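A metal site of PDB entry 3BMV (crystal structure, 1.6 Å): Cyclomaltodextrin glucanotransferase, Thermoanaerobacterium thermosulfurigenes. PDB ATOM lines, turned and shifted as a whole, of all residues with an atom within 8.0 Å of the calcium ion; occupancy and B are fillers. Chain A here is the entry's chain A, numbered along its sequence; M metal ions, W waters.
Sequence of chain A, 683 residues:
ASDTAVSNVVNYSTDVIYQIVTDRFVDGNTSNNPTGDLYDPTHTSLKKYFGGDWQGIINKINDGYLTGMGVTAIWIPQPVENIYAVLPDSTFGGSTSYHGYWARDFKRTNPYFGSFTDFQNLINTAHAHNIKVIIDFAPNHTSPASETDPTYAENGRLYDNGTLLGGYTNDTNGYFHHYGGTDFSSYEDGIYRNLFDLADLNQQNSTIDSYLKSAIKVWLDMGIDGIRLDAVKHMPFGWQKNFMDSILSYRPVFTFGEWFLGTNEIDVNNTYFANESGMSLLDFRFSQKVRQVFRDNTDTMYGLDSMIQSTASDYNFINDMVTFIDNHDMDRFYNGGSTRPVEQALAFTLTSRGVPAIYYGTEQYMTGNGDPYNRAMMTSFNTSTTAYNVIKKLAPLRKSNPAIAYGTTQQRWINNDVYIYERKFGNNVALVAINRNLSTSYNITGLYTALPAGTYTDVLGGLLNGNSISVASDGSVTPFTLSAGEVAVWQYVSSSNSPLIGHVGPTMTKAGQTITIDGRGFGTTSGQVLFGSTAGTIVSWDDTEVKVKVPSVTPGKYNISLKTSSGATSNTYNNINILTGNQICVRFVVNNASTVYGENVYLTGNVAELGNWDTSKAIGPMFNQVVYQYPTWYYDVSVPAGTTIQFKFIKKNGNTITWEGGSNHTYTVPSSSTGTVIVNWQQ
The side-chain amide oxygen of Asn 32 sits close to the backbone carbonyl oxygen of Tyr 112, 3.3 Å away. The side-chain amide nitrogen (ND2) of Asn 33 sits at hydrogen-bond distance from the side-chain hydroxyl (OH) of Tyr 39. The backbone NH of Gly 51 lies within hydrogen-bond range of the side-chain carboxylate of Asp 23, 2.9 Å away. The side-chain carboxylate of Asp 53 is in hydrogen-bond range of the backbone NH of Gly 56. The backbone NH of Asp 53 sits at hydrogen-bond distance from the backbone carbonyl oxygen of Val 26 (3.0 Å). The side-chain carboxylate of Asp 53 sits close to the backbone NH of Gln 55 (3.4 Å). OD1 of Asp 53 sits at hydrogen-bond distance from N of Gly 28 (2.8 Å). OG of Ser 31 is in hydrogen-bond range of OD1 of Asn 29, at 2.4 Å.
Within 4 Å of the calcium ion: Asp 27, Asn 29, Asn 32, Asn 33, Gly 51 and Asp 53.
The calcium ion is bound by the side-chain amide oxygen (OD1) of Asn 33 (2.3 Å). The side-chain amide oxygen (OD1) of Asn 32 binds the calcium ion (2.4 Å). The calcium ion is bound by the side-chain carboxylate (OD2) of Asp 53. O of Gly 51 is bound to the calcium ion (2.4 Å). The calcium ion is bound by OD1 of Asp 27, 2.4 Å away. The calcium ion is bound by O of Asn 29 (2.5 Å). Water W1 is bound to the calcium ion (2.5 Å). The calcium ion has seven donor atoms within binding distance.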
ATOM      1  N   THR A  22      23.017 -28.782 -26.699  1.00  0.00           N
ATOM      2  CA  THR A  22      23.813 -27.651 -26.231  1.00  0.00           C
ATOM      3  C   THR A  22      23.521 -27.237 -24.794  1.00  0.00           C
ATOM      4  O   THR A  22      24.436 -27.117 -23.978  1.00  0.00           O
ATOM      5  CB  THR A  22      23.670 -26.452 -27.187  1.00  0.00           C
ATOM      6  OG1 THR A  22      24.180 -26.818 -28.474  1.00  0.00           O
ATOM      7  CG2 THR A  22      24.434 -25.234 -26.680  1.00  0.00           C
ATOM      8  N   ASP A  23      22.239 -27.030 -24.493  1.00  0.00           N
ATOM      9  CA  ASP A  23      21.842 -26.554 -23.169  1.00  0.00           C
ATOM     10  C   ASP A  23      22.220 -27.527 -22.058  1.00  0.00           C
ATOM     11  O   ASP A  23      22.352 -27.125 -20.896  1.00  0.00           O
ATOM     12  CB  ASP A  23      20.334 -26.285 -23.112  1.00  0.00           C
ATOM     13  CG  ASP A  23      19.914 -25.697 -21.782  1.00  0.00           C
ATOM     14  OD1 ASP A  23      20.325 -24.549 -21.493  1.00  0.00           O
ATOM     15  OD2 ASP A  23      19.212 -26.398 -21.031  1.00  0.00           O
ATOM     16  N   VAL A  26      27.679 -28.342 -21.463  1.00  0.00           N
ATOM     17  CA  VAL A  26      28.549 -27.581 -20.541  1.00  0.00           C
ATOM     18  C   VAL A  26      28.184 -26.098 -20.562  1.00  0.00           C
ATOM     19  O   VAL A  26      28.156 -25.479 -21.620  1.00  0.00           O
ATOM     20  CB  VAL A  26      30.053 -27.749 -20.890  1.00  0.00           C
ATOM     21  CG1 VAL A  26      30.924 -26.872 -19.979  1.00  0.00           C
ATOM     22  CG2 VAL A  26      30.483 -29.195 -20.773  1.00  0.00           C
ATOM     23  N   ASP A  27      27.923 -25.549 -19.380  1.00  0.00           N
ATOM     24  CA  ASP A  27      27.717 -24.112 -19.213  1.00  0.00           C
ATOM     25  C   ASP A  27      29.097 -23.446 -19.156  1.00  0.00           C
ATOM     26  O   ASP A  27      29.672 -23.300 -18.084  1.00  0.00           O
ATOM     27  CB  ASP A  27      26.903 -23.862 -17.935  1.00  0.00           C
ATOM     28  CG  ASP A  27      26.585 -22.387 -17.709  1.00  0.00           C
ATOM     29  OD1 ASP A  27      26.927 -21.521 -18.543  1.00  0.00           O
ATOM     30  OD2 ASP A  27      25.981 -22.096 -16.647  1.00  0.00           O
ATOM     31  N   GLY A  28      29.621 -23.069 -20.323  1.00  0.00           N
ATOM     32  CA  GLY A  28      30.948 -22.442 -20.397  1.00  0.00           C
ATOM     33  C   GLY A  28      30.971 -20.965 -20.064  1.00  0.00           C
ATOM     34  O   GLY A  28      32.030 -20.387 -19.816  1.00  0.00           O
ATOM     35  N   ASN A  29      29.796 -20.336 -20.067  1.00  0.00           N
ATOM     36  CA  ASN A  29      29.694 -18.928 -19.697  1.00  0.00           C
ATOM     37  C   ASN A  29      28.405 -18.660 -18.938  1.00  0.00           C
ATOM     38  O   ASN A  29      27.317 -18.737 -19.507  1.00  0.00           O
ATOM     39  CB  ASN A  29      29.836 -18.006 -20.909  1.00  0.00           C
ATOM     40  CG  ASN A  29      29.853 -16.535 -20.519  1.00  0.00           C
ATOM     41  OD1 ASN A  29      28.803 -15.943 -20.291  1.00  0.00           O
ATOM     42  ND2 ASN A  29      31.039 -15.949 -20.419  1.00  0.00           N
ATOM     43  N   THR A  30      28.533 -18.348 -17.662  1.00  0.00           N
ATOM     44  CA  THR A  30      27.338 -18.110 -16.833  1.00  0.00           C
ATOM     45  C   THR A  30      26.669 -16.780 -17.140  1.00  0.00           C
ATOM     46  O   THR A  30      25.470 -16.618 -16.904  1.00  0.00           O
ATOM     47  CB  THR A  30      27.644 -18.224 -15.326  1.00  0.00           C
ATOM     48  OG1 THR A  30      28.594 -17.232 -14.946  1.00  0.00           O
ATOM     49  CG2 THR A  30      28.190 -19.614 -14.993  1.00  0.00           C
ATOM     50  N   SER A  31      27.438 -15.820 -17.669  1.00  0.00           N
ATOM     51  CA  SER A  31      26.897 -14.480 -17.921  1.00  0.00           C
ATOM     52  C   SER A  31      25.833 -14.474 -19.016  1.00  0.00           C
ATOM     53  O   SER A  31      25.027 -13.554 -19.076  1.00  0.00           O
ATOM     54  CB  SER A  31      28.006 -13.470 -18.252  1.00  0.00           C
ATOM     55  OG  SER A  31      28.432 -13.629 -19.597  1.00  0.00           O
ATOM     56  N   ASN A  32      25.856 -15.489 -19.879  1.00  0.00           N
ATOM     57  CA  ASN A  32      24.849 -15.597 -20.935  1.00  0.00           C
ATOM     58  C   ASN A  32      23.614 -16.407 -20.552  1.00  0.00           C
ATOM     59  O   ASN A  32      22.684 -16.545 -21.340  1.00  0.00           O
ATOM     60  CB  ASN A  32      25.470 -16.067 -22.259  1.00  0.00           C
ATOM     61  CG  ASN A  32      25.879 -17.540 -22.243  1.00  0.00           C
ATOM     62  OD1 ASN A  32      25.401 -18.327 -21.426  1.00  0.00           O
ATOM     63  ND2 ASN A  32      26.749 -17.921 -23.182  1.00  0.00           N
ATOM     64  N   ASN A  33      23.583 -16.932 -19.320  1.00  0.00           N
ATOM     65  CA  ASN A  33      22.437 -17.689 -18.841  1.00  0.00           C
ATOM     66  C   ASN A  33      21.164 -16.850 -18.786  1.00  0.00           C
ATOM     67  O   ASN A  33      21.233 -15.662 -18.460  1.00  0.00           O
ATOM     68  CB  ASN A  33      22.699 -18.271 -17.444  1.00  0.00           C
ATOM     69  CG  ASN A  33      23.723 -19.376 -17.461  1.00  0.00           C
ATOM     70  OD1 ASN A  33      24.138 -19.842 -18.524  1.00  0.00           O
ATOM     71  ND2 ASN A  33      24.136 -19.814 -16.275  1.00  0.00           N
ATOM     72  N   PRO A  34      20.004 -17.464 -19.093  1.00  0.00           N
ATOM     73  CA  PRO A  34      18.753 -16.734 -18.875  1.00  0.00           C
ATOM     74  C   PRO A  34      18.572 -16.388 -17.402  1.00  0.00           C
ATOM     75  O   PRO A  34      19.259 -16.941 -16.541  1.00  0.00           O
ATOM     76  CB  PRO A  34      17.673 -17.745 -19.282  1.00  0.00           C
ATOM     77  CG  PRO A  34      18.351 -18.770 -20.088  1.00  0.00           C
ATOM     78  CD  PRO A  34      19.780 -18.817 -19.640  1.00  0.00           C
ATOM     79  N   TYR A  39      15.370 -20.225 -16.453  1.00  0.00           N
ATOM     80  CA  TYR A  39      16.631 -20.851 -16.080  1.00  0.00           C
ATOM     81  C   TYR A  39      16.552 -21.629 -14.774  1.00  0.00           C
ATOM     82  O   TYR A  39      15.984 -21.144 -13.781  1.00  0.00           O
ATOM     83  CB  TYR A  39      17.712 -19.757 -15.996  1.00  0.00           C
ATOM     84  CG  TYR A  39      19.060 -20.190 -15.438  1.00  0.00           C
ATOM     85  CD1 TYR A  39      19.820 -21.156 -16.073  1.00  0.00           C
ATOM     86  CD2 TYR A  39      19.572 -19.593 -14.284  1.00  0.00           C
ATOM     87  CE1 TYR A  39      21.075 -21.547 -15.566  1.00  0.00           C
ATOM     88  CE2 TYR A  39      20.813 -19.964 -13.776  1.00  0.00           C
ATOM     89  CZ  TYR A  39      21.546 -20.938 -14.416  1.00  0.00           C
ATOM     90  OH  TYR A  39      22.774 -21.316 -13.908  1.00  0.00           O
ATOM     91  N   TYR A  49      16.002 -24.025 -19.259  1.00  0.00           N
ATOM     92  CA  TYR A  49      17.385 -23.840 -19.656  1.00  0.00           C
ATOM     93  C   TYR A  49      18.286 -24.171 -18.467  1.00  0.00           C
ATOM     94  O   TYR A  49      18.090 -23.639 -17.369  1.00  0.00           O
ATOM     95  CB  TYR A  49      17.660 -22.395 -20.054  1.00  0.00           C
ATOM     96  CG  TYR A  49      17.275 -22.011 -21.467  1.00  0.00           C
ATOM     97  CD1 TYR A  49      15.969 -21.643 -21.777  1.00  0.00           C
ATOM     98  CD2 TYR A  49      18.237 -21.987 -22.479  1.00  0.00           C
ATOM     99  CE1 TYR A  49      15.619 -21.268 -23.076  1.00  0.00           C
ATOM    100  CE2 TYR A  49      17.907 -21.605 -23.766  1.00  0.00           C
ATOM    101  CZ  TYR A  49      16.599 -21.260 -24.067  1.00  0.00           C
ATOM    102  OH  TYR A  49      16.274 -20.885 -25.349  1.00  0.00           O
ATOM    103  N   PHE A  50      19.259 -25.045 -18.697  1.00  0.00           N
ATOM    104  CA  PHE A  50      20.275 -25.372 -17.690  1.00  0.00           C
ATOM    105  C   PHE A  50      21.549 -24.532 -17.863  1.00  0.00           C
ATOM    106  O   PHE A  50      22.397 -24.495 -16.966  1.00  0.00           O
ATOM    107  CB  PHE A  50      20.618 -26.869 -17.751  1.00  0.00           C
ATOM    108  CG  PHE A  50      19.553 -27.779 -17.191  1.00  0.00           C
ATOM    109  CD1 PHE A  50      18.338 -27.272 -16.711  1.00  0.00           C
ATOM    110  CD2 PHE A  50      19.760 -29.151 -17.159  1.00  0.00           C
ATOM    111  CE1 PHE A  50      17.362 -28.121 -16.206  1.00  0.00           C
ATOM    112  CE2 PHE A  50      18.784 -30.014 -16.655  1.00  0.00           C
ATOM    113  CZ  PHE A  50      17.581 -29.500 -16.175  1.00  0.00           C
ATOM    114  N   GLY A  51      21.680 -23.868 -19.002  1.00  0.00           N
ATOM    115  CA  GLY A  51      22.771 -22.926 -19.234  1.00  0.00           C
ATOM    116  C   GLY A  51      23.898 -23.402 -20.132  1.00  0.00           C
ATOM    117  O   GLY A  51      24.849 -22.660 -20.369  1.00  0.00           O
ATOM    118  N   GLY A  52      23.802 -24.631 -20.635  1.00  0.00           N
ATOM    119  CA  GLY A  52      24.820 -25.162 -21.553  1.00  0.00           C
ATOM    120  C   GLY A  52      24.921 -24.303 -22.799  1.00  0.00           C
ATOM    121  O   GLY A  52      23.911 -23.833 -23.316  1.00  0.00           O
ATOM    122  N   ASP A  53      26.137 -24.091 -23.282  1.00  0.00           N
ATOM    123  CA  ASP A  53      26.323 -23.102 -24.355  1.00  0.00           C
ATOM    124  C   ASP A  53      27.481 -23.445 -25.287  1.00  0.00           C
ATOM    125  O   ASP A  53      28.152 -24.464 -25.106  1.00  0.00           O
ATOM    126  CB  ASP A  53      26.484 -21.695 -23.749  1.00  0.00           C
ATOM    127  CG  ASP A  53      27.579 -21.630 -22.700  1.00  0.00           C
ATOM    128  OD1 ASP A  53      28.593 -22.353 -22.847  1.00  0.00           O
ATOM    129  OD2 ASP A  53      27.426 -20.861 -21.736  1.00  0.00           O
ATOM    130  N   TRP A  54      27.714 -22.597 -26.288  1.00  0.00           N
ATOM    131  CA  TRP A  54      28.752 -22.871 -27.268  1.00  0.00           C
ATOM    132  C   TRP A  54      30.156 -22.798 -26.679  1.00  0.00           C
ATOM    133  O   TRP A  54      31.035 -23.586 -27.038  1.00  0.00           O
ATOM    134  CB  TRP A  54      28.614 -21.984 -28.510  1.00  0.00           C
ATOM    135  CG  TRP A  54      27.312 -22.229 -29.230  1.00  0.00           C
ATOM    136  CD1 TRP A  54      26.646 -23.425 -29.330  1.00  0.00           C
ATOM    137  CD2 TRP A  54      26.530 -21.270 -29.942  1.00  0.00           C
ATOM    138  NE1 TRP A  54      25.486 -23.255 -30.070  1.00  0.00           N
ATOM    139  CE2 TRP A  54      25.402 -21.946 -30.454  1.00  0.00           C
ATOM    140  CE3 TRP A  54      26.674 -19.891 -30.191  1.00  0.00           C
ATOM    141  CZ2 TRP A  54      24.409 -21.295 -31.203  1.00  0.00           C
ATOM    142  CZ3 TRP A  54      25.693 -19.246 -30.941  1.00  0.00           C
ATOM    143  CH2 TRP A  54      24.580 -19.944 -31.438  1.00  0.00           C
ATOM    144  N   GLN A  55      30.369 -21.862 -25.750  1.00  0.00           N
ATOM    145  CA  GLN A  55      31.637 -21.797 -25.024  1.00  0.00           C
ATOM    146  C   GLN A  55      31.933 -23.113 -24.305  1.00  0.00           C
ATOM    147  O   GLN A  55      33.075 -23.575 -24.284  1.00  0.00           O
ATOM    148  CB  GLN A  55      31.649 -20.622 -24.037  1.00  0.00           C
ATOM    149  CG  GLN A  55      32.987 -20.432 -23.312  1.00  0.00           C
ATOM    150  CD  GLN A  55      34.136 -20.168 -24.264  1.00  0.00           C
ATOM    151  OE1 GLN A  55      34.075 -19.269 -25.096  1.00  0.00           O
ATOM    152  NE2 GLN A  55      35.217 -20.945 -24.128  1.00  0.00           N
ATOM    153  N   GLY A  56      30.890 -23.710 -23.726  1.00  0.00           N
ATOM    154  CA  GLY A  56      31.009 -25.034 -23.095  1.00  0.00           C
ATOM    155  C   GLY A  56      31.517 -26.113 -24.024  1.00  0.00           C
ATOM    156  O   GLY A  56      32.399 -26.897 -23.651  1.00  0.00           O
ATOM    157  N   PRO A 111      20.681 -16.134 -27.953  1.00  0.00           N
ATOM    158  CA  PRO A 111      21.717 -15.463 -27.161  1.00  0.00           C
ATOM    159  C   PRO A 111      22.162 -16.286 -25.949  1.00  0.00           C
ATOM    160  O   PRO A 111      23.252 -16.055 -25.417  1.00  0.00           O
ATOM    161  CB  PRO A 111      21.046 -14.159 -26.716  1.00  0.00           C
ATOM    162  CG  PRO A 111      19.584 -14.470 -26.735  1.00  0.00           C
ATOM    163  CD  PRO A 111      19.409 -15.386 -27.912  1.00  0.00           C
ATOM    164  N   TYR A 112      21.350 -17.237 -25.528  1.00  0.00           N
ATOM    165  CA  TYR A 112      21.708 -18.078 -24.403  1.00  0.00           C
ATOM    166  C   TYR A 112      22.795 -19.079 -24.789  1.00  0.00           C
ATOM    167  O   TYR A 112      23.634 -19.448 -23.961  1.00  0.00           O
ATOM    168  CB  TYR A 112      20.475 -18.785 -23.830  1.00  0.00           C
ATOM    169  CG  TYR A 112      19.378 -17.822 -23.430  1.00  0.00           C
ATOM    170  CD1 TYR A 112      19.664 -16.721 -22.608  1.00  0.00           C
ATOM    171  CD2 TYR A 112      18.062 -17.999 -23.852  1.00  0.00           C
ATOM    172  CE1 TYR A 112      18.657 -15.829 -22.235  1.00  0.00           C
ATOM    173  CE2 TYR A 112      17.051 -17.115 -23.468  1.00  0.00           C
ATOM    174  CZ  TYR A 112      17.367 -16.032 -22.661  1.00  0.00           C
ATOM    175  OH  TYR A 112      16.385 -15.140 -22.271  1.00  0.00           O
ATOM    176  N   PHE A 113      22.786 -19.507 -26.045  1.00  0.00           N
ATOM    177  CA  PHE A 113      23.862 -20.368 -26.555  1.00  0.00           C
ATOM    178  C   PHE A 113      25.096 -19.523 -26.866  1.00  0.00           C
ATOM    179  O   PHE A 113      26.228 -19.968 -26.669  1.00  0.00           O
ATOM    180  CB  PHE A 113      23.413 -21.120 -27.819  1.00  0.00           C
ATOM    181  CG  PHE A 113      22.296 -22.111 -27.614  1.00  0.00           C
ATOM    182  CD1 PHE A 113      21.939 -22.567 -26.338  1.00  0.00           C
ATOM    183  CD2 PHE A 113      21.607 -22.608 -28.718  1.00  0.00           C
ATOM    184  CE1 PHE A 113      20.898 -23.493 -26.169  1.00  0.00           C
ATOM    185  CE2 PHE A 113      20.570 -23.539 -28.562  1.00  0.00           C
ATOM    186  CZ  PHE A 113      20.220 -23.981 -27.290  1.00  0.00           C
ATOM    187  N   GLY A 114      24.860 -18.311 -27.371  1.00  0.00           N
ATOM    188  CA  GLY A 114      25.942 -17.367 -27.632  1.00  0.00           C
ATOM    189  C   GLY A 114      25.620 -16.363 -28.730  1.00  0.00           C
ATOM    190  O   GLY A 114      24.538 -16.409 -29.319  1.00  0.00           O
HETATM  191 CA    CA M   1      25.604 -20.352 -20.235  1.00  0.00          CA
HETATM  192  O   HOH W   1      23.436 -20.322 -21.431  1.00  0.00           O
